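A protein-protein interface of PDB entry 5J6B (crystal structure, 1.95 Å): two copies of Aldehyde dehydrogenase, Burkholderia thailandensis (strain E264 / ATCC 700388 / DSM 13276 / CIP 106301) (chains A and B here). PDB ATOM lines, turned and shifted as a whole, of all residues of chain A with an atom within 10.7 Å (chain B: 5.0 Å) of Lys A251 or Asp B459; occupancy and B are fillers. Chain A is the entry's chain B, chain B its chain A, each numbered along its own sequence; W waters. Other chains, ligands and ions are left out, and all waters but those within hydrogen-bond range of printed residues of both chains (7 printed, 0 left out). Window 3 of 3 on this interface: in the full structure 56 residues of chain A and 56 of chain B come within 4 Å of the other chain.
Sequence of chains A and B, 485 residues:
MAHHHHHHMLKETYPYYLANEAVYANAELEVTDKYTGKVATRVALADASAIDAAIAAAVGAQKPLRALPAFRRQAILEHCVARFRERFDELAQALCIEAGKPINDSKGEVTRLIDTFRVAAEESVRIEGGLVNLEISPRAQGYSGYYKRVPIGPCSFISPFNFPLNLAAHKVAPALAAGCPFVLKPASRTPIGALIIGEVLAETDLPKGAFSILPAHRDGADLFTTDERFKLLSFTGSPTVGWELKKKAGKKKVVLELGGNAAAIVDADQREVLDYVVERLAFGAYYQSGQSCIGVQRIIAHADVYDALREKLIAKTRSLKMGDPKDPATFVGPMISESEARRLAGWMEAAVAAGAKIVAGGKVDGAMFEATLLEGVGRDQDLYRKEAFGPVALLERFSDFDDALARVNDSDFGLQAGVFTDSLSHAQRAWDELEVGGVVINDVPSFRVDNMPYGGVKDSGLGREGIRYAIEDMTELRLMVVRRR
The indole nitrogen of Trp B243 sits at hydrogen-bond distance from the backbone carbonyl oxygen of Asp B459, at 3.1 Å. The backbone NH (N) of Asp B459 is in hydrogen-bond range of the backbone carbonyl oxygen (O) of Asp B412 (3.0 Å). O of Asp A227 is in hydrogen-bond range of NZ of Lys A252 (3.1 Å).
Of the 24 printed residues of chain A, 5 touch a printed residue of chain B. Printed residues of chain A that touch a printed residue of chain B: Lys A231, Gly A250, Lys A251, Lys A252 and Glu A476. Along chain A the printed residues that touch a printed residue of chain B span positions 231 to 476. Along chain B the printed residues that touch a printed residue of chain A span positions 243 to 459. Among the printed residues, 7 pairs touch across the chains. Among the printed residues, Asp or Glu carboxylates within 4 Å of a Lys or Arg side-chain nitrogen of the other chain: Lys A251 with Asp B459 (2.7 Å).
The side-chain amino group of Lys B246 lies within hydrogen-bond range of the backbone carbonyl oxygen of Gly A250 (2.9 Å). NZ of Lys B246 sits at hydrogen-bond distance from O of Lys A252, at 2.7 Å. NZ of Lys A251 is in salt-bridge range of OD1 of Asp B459.
Of the printed residues of chain B, Lys A251 touches Trp B243 (3.3 Å), Lys B246 (3.6 Å) and Asp B459 (2.7 Å). Asp B459 touches just one residue of chain A: Lys A251 (2.7 Å). No residue of chain A comes within 4 Å of Asp B412. No residue of chain A comes within 4 Å of Phe B413. No residue of chain A comes within 4 Å of Ser B460. No residue of chain A comes within 4 Å of Gly B461. Printed residues of chain B within 4 Å of Glu A476: Val B457. Of the printed residues of chain A, Trp B243 touches Lys A251 (3.3 Å). Of the printed residues of chain A, Val B457 touches Glu A476 (3.8 Å). Lys A248 touches none of the printed residues of chain B. The nearest residue of chain A that does not touch Asp B459 is Lys A231 (5.5 Å). The nearest printed residue of chain B that does not touch Gly A250 is Trp B243 (5.2 Å).
Water W7 bridges the backbone carbonyl oxygen of Trp B243 (2.6 Å) and the backbone carbonyl oxygen of Gly A250 (3.2 Å). Water W1 bridges the side-chain carboxylate of Asp B459 and the side-chain amino group of Lys A231. Water W3 lies within hydrogen-bond range of the backbone carbonyl oxygen of Lys A246 (2.7 Å) and the side-chain amino group of Lys B246 (3.0 Å).
1 position is printed for both chains. Of the 7 pairs that touch across the chains among the printed residues, none has its exchanged pair printed and touching as well.
Lys A231 touches Lys B458. Lys A251 touches Trp B243 (O to CZ3, 3.3 Å). O of Lys A251 touches CE of Lys B246 (3.6 Å). Glu A476 touches Val B457.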
ATOM      1  N   ILE A 152      22.376 -37.615  16.272  1.00  0.00           N
ATOM      2  CA  ILE A 152      22.870 -36.342  15.761  1.00  0.00           C
ATOM      3  C   ILE A 152      21.705 -35.379  15.523  1.00  0.00           C
ATOM      4  O   ILE A 152      21.859 -34.156  15.664  1.00  0.00           O
ATOM      5  CB  ILE A 152      23.717 -36.552  14.486  1.00  0.00           C
ATOM      6  CG1 ILE A 152      24.556 -35.295  14.209  1.00  0.00           C
ATOM      7  CG2 ILE A 152      22.816 -36.937  13.270  1.00  0.00           C
ATOM      8  CD1 ILE A 152      25.530 -35.416  13.037  1.00  0.00           C
ATOM      9  N   PRO A 154      17.940 -34.746  12.915  1.00  0.00           N
ATOM     10  CA  PRO A 154      17.321 -35.139  11.641  1.00  0.00           C
ATOM     11  C   PRO A 154      18.354 -35.334  10.539  1.00  0.00           C
ATOM     12  O   PRO A 154      19.285 -34.539  10.377  1.00  0.00           O
ATOM     13  CB  PRO A 154      16.387 -33.965  11.327  1.00  0.00           C
ATOM     14  CG  PRO A 154      16.148 -33.297  12.657  1.00  0.00           C
ATOM     15  CD  PRO A 154      17.468 -33.433  13.375  1.00  0.00           C
ATOM     16  N   PHE A 224      16.972 -30.888   0.481  1.00  0.00           N
ATOM     17  CA  PHE A 224      17.675 -32.027   1.080  1.00  0.00           C
ATOM     18  C   PHE A 224      19.139 -31.713   1.369  1.00  0.00           C
ATOM     19  O   PHE A 224      19.750 -32.363   2.226  1.00  0.00           O
ATOM     20  CB  PHE A 224      17.596 -33.250   0.173  1.00  0.00           C
ATOM     21  CG  PHE A 224      16.248 -33.928   0.181  1.00  0.00           C
ATOM     22  CD1 PHE A 224      15.268 -33.576  -0.740  1.00  0.00           C
ATOM     23  CD2 PHE A 224      15.965 -34.923   1.119  1.00  0.00           C
ATOM     24  CE1 PHE A 224      14.017 -34.226  -0.727  1.00  0.00           C
ATOM     25  CE2 PHE A 224      14.747 -35.565   1.133  1.00  0.00           C
ATOM     26  CZ  PHE A 224      13.769 -35.212   0.215  1.00  0.00           C
ATOM     27  N   THR A 225      19.713 -30.746   0.665  1.00  0.00           N
ATOM     28  CA  THR A 225      21.074 -30.305   0.948  1.00  0.00           C
ATOM     29  C   THR A 225      21.130 -29.065   1.831  1.00  0.00           C
ATOM     30  O   THR A 225      21.962 -29.001   2.743  1.00  0.00           O
ATOM     31  CB  THR A 225      21.829 -30.029  -0.361  1.00  0.00           C
ATOM     32  OG1 THR A 225      21.885 -31.229  -1.141  1.00  0.00           O
ATOM     33  CG2 THR A 225      23.253 -29.566  -0.073  1.00  0.00           C
ATOM     34  N   THR A 226      20.261 -28.079   1.599  1.00  0.00           N
ATOM     35  CA  THR A 226      20.449 -26.768   2.208  1.00  0.00           C
ATOM     36  C   THR A 226      19.682 -26.544   3.505  1.00  0.00           C
ATOM     37  O   THR A 226      20.021 -25.606   4.233  1.00  0.00           O
ATOM     38  CB  THR A 226      20.061 -25.644   1.229  1.00  0.00           C
ATOM     39  OG1 THR A 226      18.664 -25.723   0.918  1.00  0.00           O
ATOM     40  CG2 THR A 226      20.897 -25.715  -0.062  1.00  0.00           C
ATOM     41  N   ASP A 227      18.644 -27.323   3.814  1.00  0.00           N
ATOM     42  CA  ASP A 227      17.840 -26.974   4.983  1.00  0.00           C
ATOM     43  C   ASP A 227      18.654 -27.159   6.262  1.00  0.00           C
ATOM     44  O   ASP A 227      19.173 -28.245   6.521  1.00  0.00           O
ATOM     45  CB  ASP A 227      16.573 -27.807   5.058  1.00  0.00           C
ATOM     46  CG  ASP A 227      15.546 -27.189   5.988  1.00  0.00           C
ATOM     47  OD1 ASP A 227      14.563 -26.613   5.487  1.00  0.00           O
ATOM     48  OD2 ASP A 227      15.745 -27.235   7.215  1.00  0.00           O
ATOM     49  N   GLU A 228      18.745 -26.100   7.074  1.00  0.00           N
ATOM     50  CA  GLU A 228      19.590 -26.144   8.264  1.00  0.00           C
ATOM     51  C   GLU A 228      18.979 -26.935   9.414  1.00  0.00           C
ATOM     52  O   GLU A 228      19.655 -27.119  10.434  1.00  0.00           O
ATOM     53  CB  GLU A 228      19.919 -24.717   8.733  1.00  0.00           C
ATOM     54  CG  GLU A 228      20.779 -23.931   7.739  1.00  0.00           C
ATOM     55  CD  GLU A 228      22.254 -23.838   8.148  1.00  0.00           C
ATOM     56  OE1 GLU A 228      22.591 -22.916   8.933  1.00  0.00           O
ATOM     57  OE2 GLU A 228      23.072 -24.674   7.684  1.00  0.00           O
ATOM     58  N   ARG A 229      17.729 -27.402   9.289  1.00  0.00           N
ATOM     59  CA  ARG A 229      17.179 -28.287  10.311  1.00  0.00           C
ATOM     60  C   ARG A 229      17.732 -29.709  10.225  1.00  0.00           C
ATOM     61  O   ARG A 229      17.660 -30.441  11.219  1.00  0.00           O
ATOM     62  CB  ARG A 229      15.642 -28.312  10.235  1.00  0.00           C
ATOM     63  CG  ARG A 229      15.001 -27.031  10.763  1.00  0.00           C
ATOM     64  CD  ARG A 229      13.535 -26.941  10.371  1.00  0.00           C
ATOM     65  NE  ARG A 229      13.363 -26.897   8.922  1.00  0.00           N
ATOM     66  CZ  ARG A 229      12.184 -26.837   8.315  1.00  0.00           C
ATOM     67  NH1 ARG A 229      11.068 -26.803   9.035  1.00  0.00           N
ATOM     68  NH2 ARG A 229      12.120 -26.803   6.986  1.00  0.00           N
ATOM     69  N   PHE A 230      18.273 -30.116   9.075  1.00  0.00           N
ATOM     70  CA  PHE A 230      19.028 -31.364   9.004  1.00  0.00           C
ATOM     71  C   PHE A 230      20.384 -31.186   9.679  1.00  0.00           C
ATOM     72  O   PHE A 230      21.051 -30.166   9.503  1.00  0.00           O
ATOM     73  CB  PHE A 230      19.269 -31.795   7.550  1.00  0.00           C
ATOM     74  CG  PHE A 230      18.041 -32.246   6.796  1.00  0.00           C
ATOM     75  CD1 PHE A 230      17.316 -33.365   7.211  1.00  0.00           C
ATOM     76  CD2 PHE A 230      17.659 -31.600   5.621  1.00  0.00           C
ATOM     77  CE1 PHE A 230      16.212 -33.809   6.478  1.00  0.00           C
ATOM     78  CE2 PHE A 230      16.544 -32.028   4.886  1.00  0.00           C
ATOM     79  CZ  PHE A 230      15.824 -33.138   5.312  1.00  0.00           C
ATOM     80  N   LYS A 231      20.805 -32.198  10.437  1.00  0.00           N
ATOM     81  CA  LYS A 231      22.117 -32.194  11.083  1.00  0.00           C
ATOM     82  C   LYS A 231      23.134 -33.051  10.342  1.00  0.00           C
ATOM     83  O   LYS A 231      24.343 -32.962  10.628  1.00  0.00           O
ATOM     84  CB  LYS A 231      21.991 -32.687  12.533  1.00  0.00           C
ATOM     85  CG  LYS A 231      21.280 -31.700  13.446  1.00  0.00           C
ATOM     86  CD  LYS A 231      22.179 -30.494  13.703  1.00  0.00           C
ATOM     87  CE  LYS A 231      21.511 -29.455  14.588  1.00  0.00           C
ATOM     88  NZ  LYS A 231      22.469 -28.343  14.875  1.00  0.00           N
ATOM     89  N   LEU A 232      22.673 -33.852   9.385  1.00  0.00           N
ATOM     90  CA  LEU A 232      23.518 -34.751   8.621  1.00  0.00           C
ATOM     91  C   LEU A 232      22.942 -34.864   7.219  1.00  0.00           C
ATOM     92  O   LEU A 232      21.726 -35.018   7.059  1.00  0.00           O
ATOM     93  CB  LEU A 232      23.586 -36.137   9.283  1.00  0.00           C
ATOM     94  CG  LEU A 232      24.192 -37.263   8.440  1.00  0.00           C
ATOM     95  CD1 LEU A 232      25.679 -36.995   8.180  1.00  0.00           C
ATOM     96  CD2 LEU A 232      24.007 -38.586   9.159  1.00  0.00           C
ATOM     97  N   LEU A 233      23.809 -34.766   6.219  1.00  0.00           N
ATOM     98  CA  LEU A 233      23.498 -35.143   4.844  1.00  0.00           C
ATOM     99  C   LEU A 233      24.333 -36.367   4.526  1.00  0.00           C
ATOM    100  O   LEU A 233      25.558 -36.328   4.660  1.00  0.00           O
ATOM    101  CB  LEU A 233      23.821 -34.017   3.859  1.00  0.00           C
ATOM    102  CG  LEU A 233      23.784 -34.408   2.372  1.00  0.00           C
ATOM    103  CD1 LEU A 233      22.404 -34.920   1.959  1.00  0.00           C
ATOM    104  CD2 LEU A 233      24.207 -33.230   1.510  1.00  0.00           C
ATOM    105  N   LEU A 245      27.264 -31.173  -3.777  1.00  0.00           N
ATOM    106  CA  LEU A 245      26.339 -31.045  -2.656  1.00  0.00           C
ATOM    107  C   LEU A 245      27.071 -30.703  -1.363  1.00  0.00           C
ATOM    108  O   LEU A 245      26.525 -29.972  -0.527  1.00  0.00           O
ATOM    109  CB  LEU A 245      25.526 -32.334  -2.472  1.00  0.00           C
ATOM    110  CG  LEU A 245      24.606 -32.734  -3.629  1.00  0.00           C
ATOM    111  CD1 LEU A 245      23.747 -33.934  -3.259  1.00  0.00           C
ATOM    112  CD2 LEU A 245      23.740 -31.551  -4.067  1.00  0.00           C
ATOM    113  N   LYS A 246      28.290 -31.226  -1.170  1.00  0.00           N
ATOM    114  CA  LYS A 246      29.032 -30.890   0.043  1.00  0.00           C
ATOM    115  C   LYS A 246      29.243 -29.384   0.144  1.00  0.00           C
ATOM    116  O   LYS A 246      29.140 -28.806   1.234  1.00  0.00           O
ATOM    117  CB  LYS A 246      30.377 -31.629   0.088  1.00  0.00           C
ATOM    118  CG  LYS A 246      31.218 -31.320   1.352  1.00  0.00           C
ATOM    119  CD  LYS A 246      32.516 -32.153   1.389  1.00  0.00           C
ATOM    120  CE  LYS A 246      33.239 -32.022   2.733  1.00  0.00           C
ATOM    121  NZ  LYS A 246      33.942 -30.706   2.858  1.00  0.00           N
ATOM    122  N   LYS A 247      29.499 -28.723  -0.992  1.00  0.00           N
ATOM    123  CA  LYS A 247      29.776 -27.291  -0.970  1.00  0.00           C
ATOM    124  C   LYS A 247      28.558 -26.463  -0.565  1.00  0.00           C
ATOM    125  O   LYS A 247      28.724 -25.342  -0.069  1.00  0.00           O
ATOM    126  CB  LYS A 247      30.298 -26.838  -2.338  1.00  0.00           C
ATOM    127  N   LYS A 248      27.347 -26.990  -0.740  1.00  0.00           N
ATOM    128  CA  LYS A 248      26.122 -26.257  -0.442  1.00  0.00           C
ATOM    129  C   LYS A 248      25.445 -26.729   0.841  1.00  0.00           C
ATOM    130  O   LYS A 248      24.352 -26.249   1.169  1.00  0.00           O
ATOM    131  CB  LYS A 248      25.149 -26.381  -1.616  1.00  0.00           C
ATOM    132  N   ALA A 249      26.073 -27.642   1.588  1.00  0.00           N
ATOM    133  CA  ALA A 249      25.391 -28.290   2.703  1.00  0.00           C
ATOM    134  C   ALA A 249      25.224 -27.387   3.930  1.00  0.00           C
ATOM    135  O   ALA A 249      24.394 -27.694   4.790  1.00  0.00           O
ATOM    136  CB  ALA A 249      26.140 -29.566   3.094  1.00  0.00           C
ATOM    137  N   GLY A 250      25.983 -26.298   4.041  1.00  0.00           N
ATOM    138  CA  GLY A 250      25.885 -25.452   5.216  1.00  0.00           C
ATOM    139  C   GLY A 250      26.555 -26.042   6.448  1.00  0.00           C
ATOM    140  O   GLY A 250      27.668 -26.560   6.360  1.00  0.00           O
ATOM    141  N   LYS A 251      25.886 -25.983   7.607  1.00  0.00           N
ATOM    142  CA  LYS A 251      26.520 -26.404   8.856  1.00  0.00           C
ATOM    143  C   LYS A 251      26.513 -27.914   9.066  1.00  0.00           C
ATOM    144  O   LYS A 251      27.323 -28.419   9.853  1.00  0.00           O
ATOM    145  CB  LYS A 251      25.822 -25.751  10.051  1.00  0.00           C
ATOM    146  CG  LYS A 251      25.837 -24.221  10.031  1.00  0.00           C
ATOM    147  CD  LYS A 251      25.196 -23.688  11.298  1.00  0.00           C
ATOM    148  CE  LYS A 251      25.183 -22.170  11.329  1.00  0.00           C
ATOM    149  NZ  LYS A 251      24.402 -21.708  12.495  1.00  0.00           N
ATOM    150  N   LYS A 252      25.630 -28.639   8.384  1.00  0.00           N
ATOM    151  CA  LYS A 252      25.431 -30.050   8.671  1.00  0.00           C
ATOM    152  C   LYS A 252      26.678 -30.878   8.359  1.00  0.00           C
ATOM    153  O   LYS A 252      27.491 -30.535   7.497  1.00  0.00           O
ATOM    154  CB  LYS A 252      24.227 -30.579   7.877  1.00  0.00           C
ATOM    155  CG  LYS A 252      24.370 -30.404   6.376  1.00  0.00           C
ATOM    156  CD  LYS A 252      23.171 -30.949   5.615  1.00  0.00           C
ATOM    157  CE  LYS A 252      21.917 -30.134   5.889  1.00  0.00           C
ATOM    158  NZ  LYS A 252      22.044 -28.705   5.488  1.00  0.00           N
ATOM    159  N   LYS A 253      26.826 -31.981   9.094  1.00  0.00           N
ATOM    160  CA  LYS A 253      27.819 -32.992   8.764  1.00  0.00           C
ATOM    161  C   LYS A 253      27.489 -33.606   7.407  1.00  0.00           C
ATOM    162  O   LYS A 253      26.318 -33.760   7.042  1.00  0.00           O
ATOM    163  CB  LYS A 253      27.839 -34.066   9.854  1.00  0.00           C
ATOM    164  CG  LYS A 253      28.823 -35.193   9.630  1.00  0.00           C
ATOM    165  CD  LYS A 253      28.805 -36.133  10.819  1.00  0.00           C
ATOM    166  CE  LYS A 253      29.797 -37.264  10.648  1.00  0.00           C
ATOM    167  NZ  LYS A 253      31.160 -36.766  10.334  1.00  0.00           N
ATOM    168  N   VAL A 254      28.525 -33.957   6.646  1.00  0.00           N
ATOM    169  CA  VAL A 254      28.345 -34.510   5.305  1.00  0.00           C
ATOM    170  C   VAL A 254      29.015 -35.877   5.233  1.00  0.00           C
ATOM    171  O   VAL A 254      30.175 -36.027   5.628  1.00  0.00           O
ATOM    172  CB  VAL A 254      28.910 -33.565   4.225  1.00  0.00           C
ATOM    173  CG1 VAL A 254      28.799 -34.201   2.837  1.00  0.00           C
ATOM    174  CG2 VAL A 254      28.169 -32.235   4.252  1.00  0.00           C
ATOM    175  N   VAL A 255      28.287 -36.872   4.723  1.00  0.00           N
ATOM    176  CA  VAL A 255      28.840 -38.195   4.438  1.00  0.00           C
ATOM    177  C   VAL A 255      28.622 -38.465   2.959  1.00  0.00           C
ATOM    178  O   VAL A 255      27.523 -38.239   2.446  1.00  0.00           O
ATOM    179  CB  VAL A 255      28.187 -39.286   5.316  1.00  0.00           C
ATOM    180  CG1 VAL A 255      28.577 -40.697   4.829  1.00  0.00           C
ATOM    181  CG2 VAL A 255      28.583 -39.097   6.785  1.00  0.00           C
ATOM    182  N   GLU A 476      26.345 -38.358  18.200  1.00  0.00           N
ATOM    183  CA  GLU A 476      27.327 -37.472  18.806  1.00  0.00           C
ATOM    184  C   GLU A 476      27.712 -38.049  20.158  1.00  0.00           C
ATOM    185  O   GLU A 476      26.874 -38.654  20.836  1.00  0.00           O
ATOM    186  CB  GLU A 476      26.764 -36.051  18.985  1.00  0.00           C
ATOM    187  CG  GLU A 476      26.657 -35.246  17.694  1.00  0.00           C
ATOM    188  CD  GLU A 476      27.999 -34.610  17.308  1.00  0.00           C
ATOM    189  OE1 GLU A 476      28.967 -34.736  18.088  1.00  0.00           O
ATOM    190  OE2 GLU A 476      28.077 -33.983  16.234  1.00  0.00           O
ATOM    191  N   PRO B 239      32.737 -18.947  16.335  1.00  0.00           N
ATOM    192  CA  PRO B 239      31.672 -19.562  15.524  1.00  0.00           C
ATOM    193  C   PRO B 239      31.443 -18.865  14.197  1.00  0.00           C
ATOM    194  O   PRO B 239      31.283 -19.539  13.173  1.00  0.00           O
ATOM    195  CB  PRO B 239      30.436 -19.449  16.430  1.00  0.00           C
ATOM    196  CG  PRO B 239      30.984 -19.390  17.810  1.00  0.00           C
ATOM    197  CD  PRO B 239      32.299 -18.648  17.709  1.00  0.00           C
ATOM    198  N   TRP B 243      32.017 -21.454  10.827  1.00  0.00           N
ATOM    199  CA  TRP B 243      30.972 -21.927   9.923  1.00  0.00           C
ATOM    200  C   TRP B 243      31.140 -21.345   8.526  1.00  0.00           C
ATOM    201  O   TRP B 243      30.775 -21.996   7.540  1.00  0.00           O
ATOM    202  CB  TRP B 243      29.577 -21.619  10.482  1.00  0.00           C
ATOM    203  CG  TRP B 243      29.291 -22.362  11.763  1.00  0.00           C
ATOM    204  CD1 TRP B 243      29.120 -21.817  13.014  1.00  0.00           C
ATOM    205  CD2 TRP B 243      29.182 -23.786  11.930  1.00  0.00           C
ATOM    206  NE1 TRP B 243      28.869 -22.816  13.933  1.00  0.00           N
ATOM    207  CE2 TRP B 243      28.926 -24.029  13.303  1.00  0.00           C
ATOM    208  CE3 TRP B 243      29.265 -24.876  11.055  1.00  0.00           C
ATOM    209  CZ2 TRP B 243      28.743 -25.323  13.819  1.00  0.00           C
ATOM    210  CZ3 TRP B 243      29.084 -26.160  11.566  1.00  0.00           C
ATOM    211  CH2 TRP B 243      28.826 -26.371  12.939  1.00  0.00           C
ATOM    212  N   LYS B 246      33.930 -23.554   6.804  1.00  0.00           N
ATOM    213  CA  LYS B 246      33.367 -24.818   6.343  1.00  0.00           C
ATOM    214  C   LYS B 246      32.748 -24.668   4.956  1.00  0.00           C
ATOM    215  O   LYS B 246      32.923 -25.541   4.096  1.00  0.00           O
ATOM    216  CB  LYS B 246      32.337 -25.335   7.357  1.00  0.00           C
ATOM    217  CG  LYS B 246      31.661 -26.656   6.960  1.00  0.00           C
ATOM    218  CD  LYS B 246      30.689 -27.130   8.056  1.00  0.00           C
ATOM    219  CE  LYS B 246      30.262 -28.591   7.864  1.00  0.00           C
ATOM    220  NZ  LYS B 246      29.398 -28.824   6.672  1.00  0.00           N
ATOM    221  N   LEU B 258      34.615 -24.327  18.356  1.00  0.00           N
ATOM    222  CA  LEU B 258      34.098 -22.962  18.409  1.00  0.00           C
ATOM    223  C   LEU B 258      33.811 -22.544  19.864  1.00  0.00           C
ATOM    224  O   LEU B 258      34.444 -23.062  20.798  1.00  0.00           O
ATOM    225  CB  LEU B 258      32.886 -22.871  17.478  1.00  0.00           C
ATOM    226  CG  LEU B 258      33.107 -23.491  16.084  1.00  0.00           C
ATOM    227  CD1 LEU B 258      31.803 -23.515  15.243  1.00  0.00           C
ATOM    228  CD2 LEU B 258      34.195 -22.742  15.334  1.00  0.00           C
ATOM    229  N   GLY B 259      32.894 -21.597  20.055  1.00  0.00           N
ATOM    230  CA  GLY B 259      32.612 -21.075  21.382  1.00  0.00           C
ATOM    231  C   GLY B 259      31.173 -21.237  21.846  1.00  0.00           C
ATOM    232  O   GLY B 259      30.428 -22.042  21.279  1.00  0.00           O
ATOM    233  N   ASP B 412      21.884 -20.768  21.142  1.00  0.00           N
ATOM    234  CA  ASP B 412      22.415 -21.253  19.875  1.00  0.00           C
ATOM    235  C   ASP B 412      23.549 -22.250  20.075  1.00  0.00           C
ATOM    236  O   ASP B 412      23.876 -22.992  19.139  1.00  0.00           O
ATOM    237  CB  ASP B 412      22.960 -20.096  19.025  1.00  0.00           C
ATOM    238  CG  ASP B 412      21.890 -19.131  18.596  1.00  0.00           C
ATOM    239  OD1 ASP B 412      20.726 -19.561  18.461  1.00  0.00           O
ATOM    240  OD2 ASP B 412      22.232 -17.949  18.383  1.00  0.00           O
ATOM    241  N   PHE B 413      24.167 -22.262  21.252  1.00  0.00           N
ATOM    242  CA  PHE B 413      25.429 -22.959  21.481  1.00  0.00           C
ATOM    243  C   PHE B 413      25.216 -24.233  22.304  1.00  0.00           C
ATOM    244  O   PHE B 413      24.108 -24.552  22.742  1.00  0.00           O
ATOM    245  CB  PHE B 413      26.424 -21.994  22.137  1.00  0.00           C
ATOM    246  CG  PHE B 413      26.629 -20.727  21.343  1.00  0.00           C
ATOM    247  CD1 PHE B 413      27.308 -20.759  20.134  1.00  0.00           C
ATOM    248  CD2 PHE B 413      26.116 -19.515  21.787  1.00  0.00           C
ATOM    249  CE1 PHE B 413      27.509 -19.592  19.394  1.00  0.00           C
ATOM    250  CE2 PHE B 413      26.303 -18.343  21.049  1.00  0.00           C
ATOM    251  CZ  PHE B 413      26.998 -18.383  19.848  1.00  0.00           C
ATOM    252  N   VAL B 457      28.315 -29.208  20.115  1.00  0.00           N
ATOM    253  CA  VAL B 457      27.241 -29.457  19.161  1.00  0.00           C
ATOM    254  C   VAL B 457      26.523 -28.134  18.929  1.00  0.00           C
ATOM    255  O   VAL B 457      26.983 -27.084  19.396  1.00  0.00           O
ATOM    256  CB  VAL B 457      26.286 -30.565  19.649  1.00  0.00           C
ATOM    257  CG1 VAL B 457      27.038 -31.886  19.740  1.00  0.00           C
ATOM    258  CG2 VAL B 457      25.653 -30.200  21.001  1.00  0.00           C
ATOM    259  N   LYS B 458      25.407 -28.169  18.191  1.00  0.00           N
ATOM    260  CA  LYS B 458      24.707 -26.950  17.789  1.00  0.00           C
ATOM    261  C   LYS B 458      25.726 -25.999  17.159  1.00  0.00           C
ATOM    262  O   LYS B 458      26.533 -26.436  16.336  1.00  0.00           O
ATOM    263  CB  LYS B 458      23.964 -26.347  18.990  1.00  0.00           C
ATOM    264  CG  LYS B 458      22.867 -27.297  19.512  1.00  0.00           C
ATOM    265  CD  LYS B 458      22.414 -26.975  20.928  1.00  0.00           C
ATOM    266  CE  LYS B 458      21.525 -25.764  20.968  1.00  0.00           C
ATOM    267  NZ  LYS B 458      21.046 -25.438  22.340  1.00  0.00           N
ATOM    268  N   ASP B 459      25.712 -24.711  17.507  1.00  0.00           N
ATOM    269  CA  ASP B 459      26.617 -23.780  16.821  1.00  0.00           C
ATOM    270  C   ASP B 459      28.019 -23.757  17.419  1.00  0.00           C
ATOM    271  O   ASP B 459      28.830 -22.917  16.998  1.00  0.00           O
ATOM    272  CB  ASP B 459      26.055 -22.360  16.817  1.00  0.00           C
ATOM    273  CG  ASP B 459      25.045 -22.146  15.715  1.00  0.00           C
ATOM    274  OD1 ASP B 459      24.938 -23.025  14.835  1.00  0.00           O
ATOM    275  OD2 ASP B 459      24.370 -21.102  15.723  1.00  0.00           O
ATOM    276  N   SER B 460      28.323 -24.657  18.354  1.00  0.00           N
ATOM    277  CA  SER B 460      29.586 -24.643  19.098  1.00  0.00           C
ATOM    278  C   SER B 460      30.673 -25.529  18.496  1.00  0.00           C
ATOM    279  O   SER B 460      31.828 -25.458  18.945  1.00  0.00           O
ATOM    280  CB  SER B 460      29.358 -25.063  20.556  1.00  0.00           C
ATOM    281  OG  SER B 460      28.706 -24.034  21.291  1.00  0.00           O
ATOM    282  N   GLY B 461      30.372 -26.352  17.503  1.00  0.00           N
ATOM    283  CA  GLY B 461      31.442 -27.137  16.922  1.00  0.00           C
ATOM    284  C   GLY B 461      30.928 -28.250  16.043  1.00  0.00           C
ATOM    285  O   GLY B 461      29.718 -28.443  15.864  1.00  0.00           O
ATOM    286  N   LEU B 462      31.897 -28.979  15.491  1.00  0.00           N
ATOM    287  CA  LEU B 462      31.654 -30.166  14.676  1.00  0.00           C
ATOM    288  C   LEU B 462      32.883 -31.056  14.804  1.00  0.00           C
ATOM    289  O   LEU B 462      33.923 -30.754  14.212  1.00  0.00           O
ATOM    290  CB  LEU B 462      31.400 -29.794  13.217  1.00  0.00           C
ATOM    291  CG  LEU B 462      30.845 -30.915  12.338  1.00  0.00           C
ATOM    292  CD1 LEU B 462      29.516 -31.426  12.909  1.00  0.00           C
ATOM    293  CD2 LEU B 462      30.678 -30.435  10.904  1.00  0.00           C
HETATM  294  O   HOH W   1      23.681 -25.379  14.548  1.00  0.00           O
HETATM  295  O   HOH W   2      22.146 -21.222  14.164  1.00  0.00           O
HETATM  296  O   HOH W   3      29.901 -28.187   3.784  1.00  0.00           O
HETATM  297  O   HOH W   4      32.536 -28.265   3.165  1.00  0.00           O
HETATM  298  O   HOH W   5      31.912 -30.590   5.434  1.00  0.00           O
HETATM  299  O   HOH W   6      23.366 -30.171  17.238  1.00  0.00           O
HETATM  300  O   HOH W   7      28.784 -23.719   7.291  1.00  0.00           O
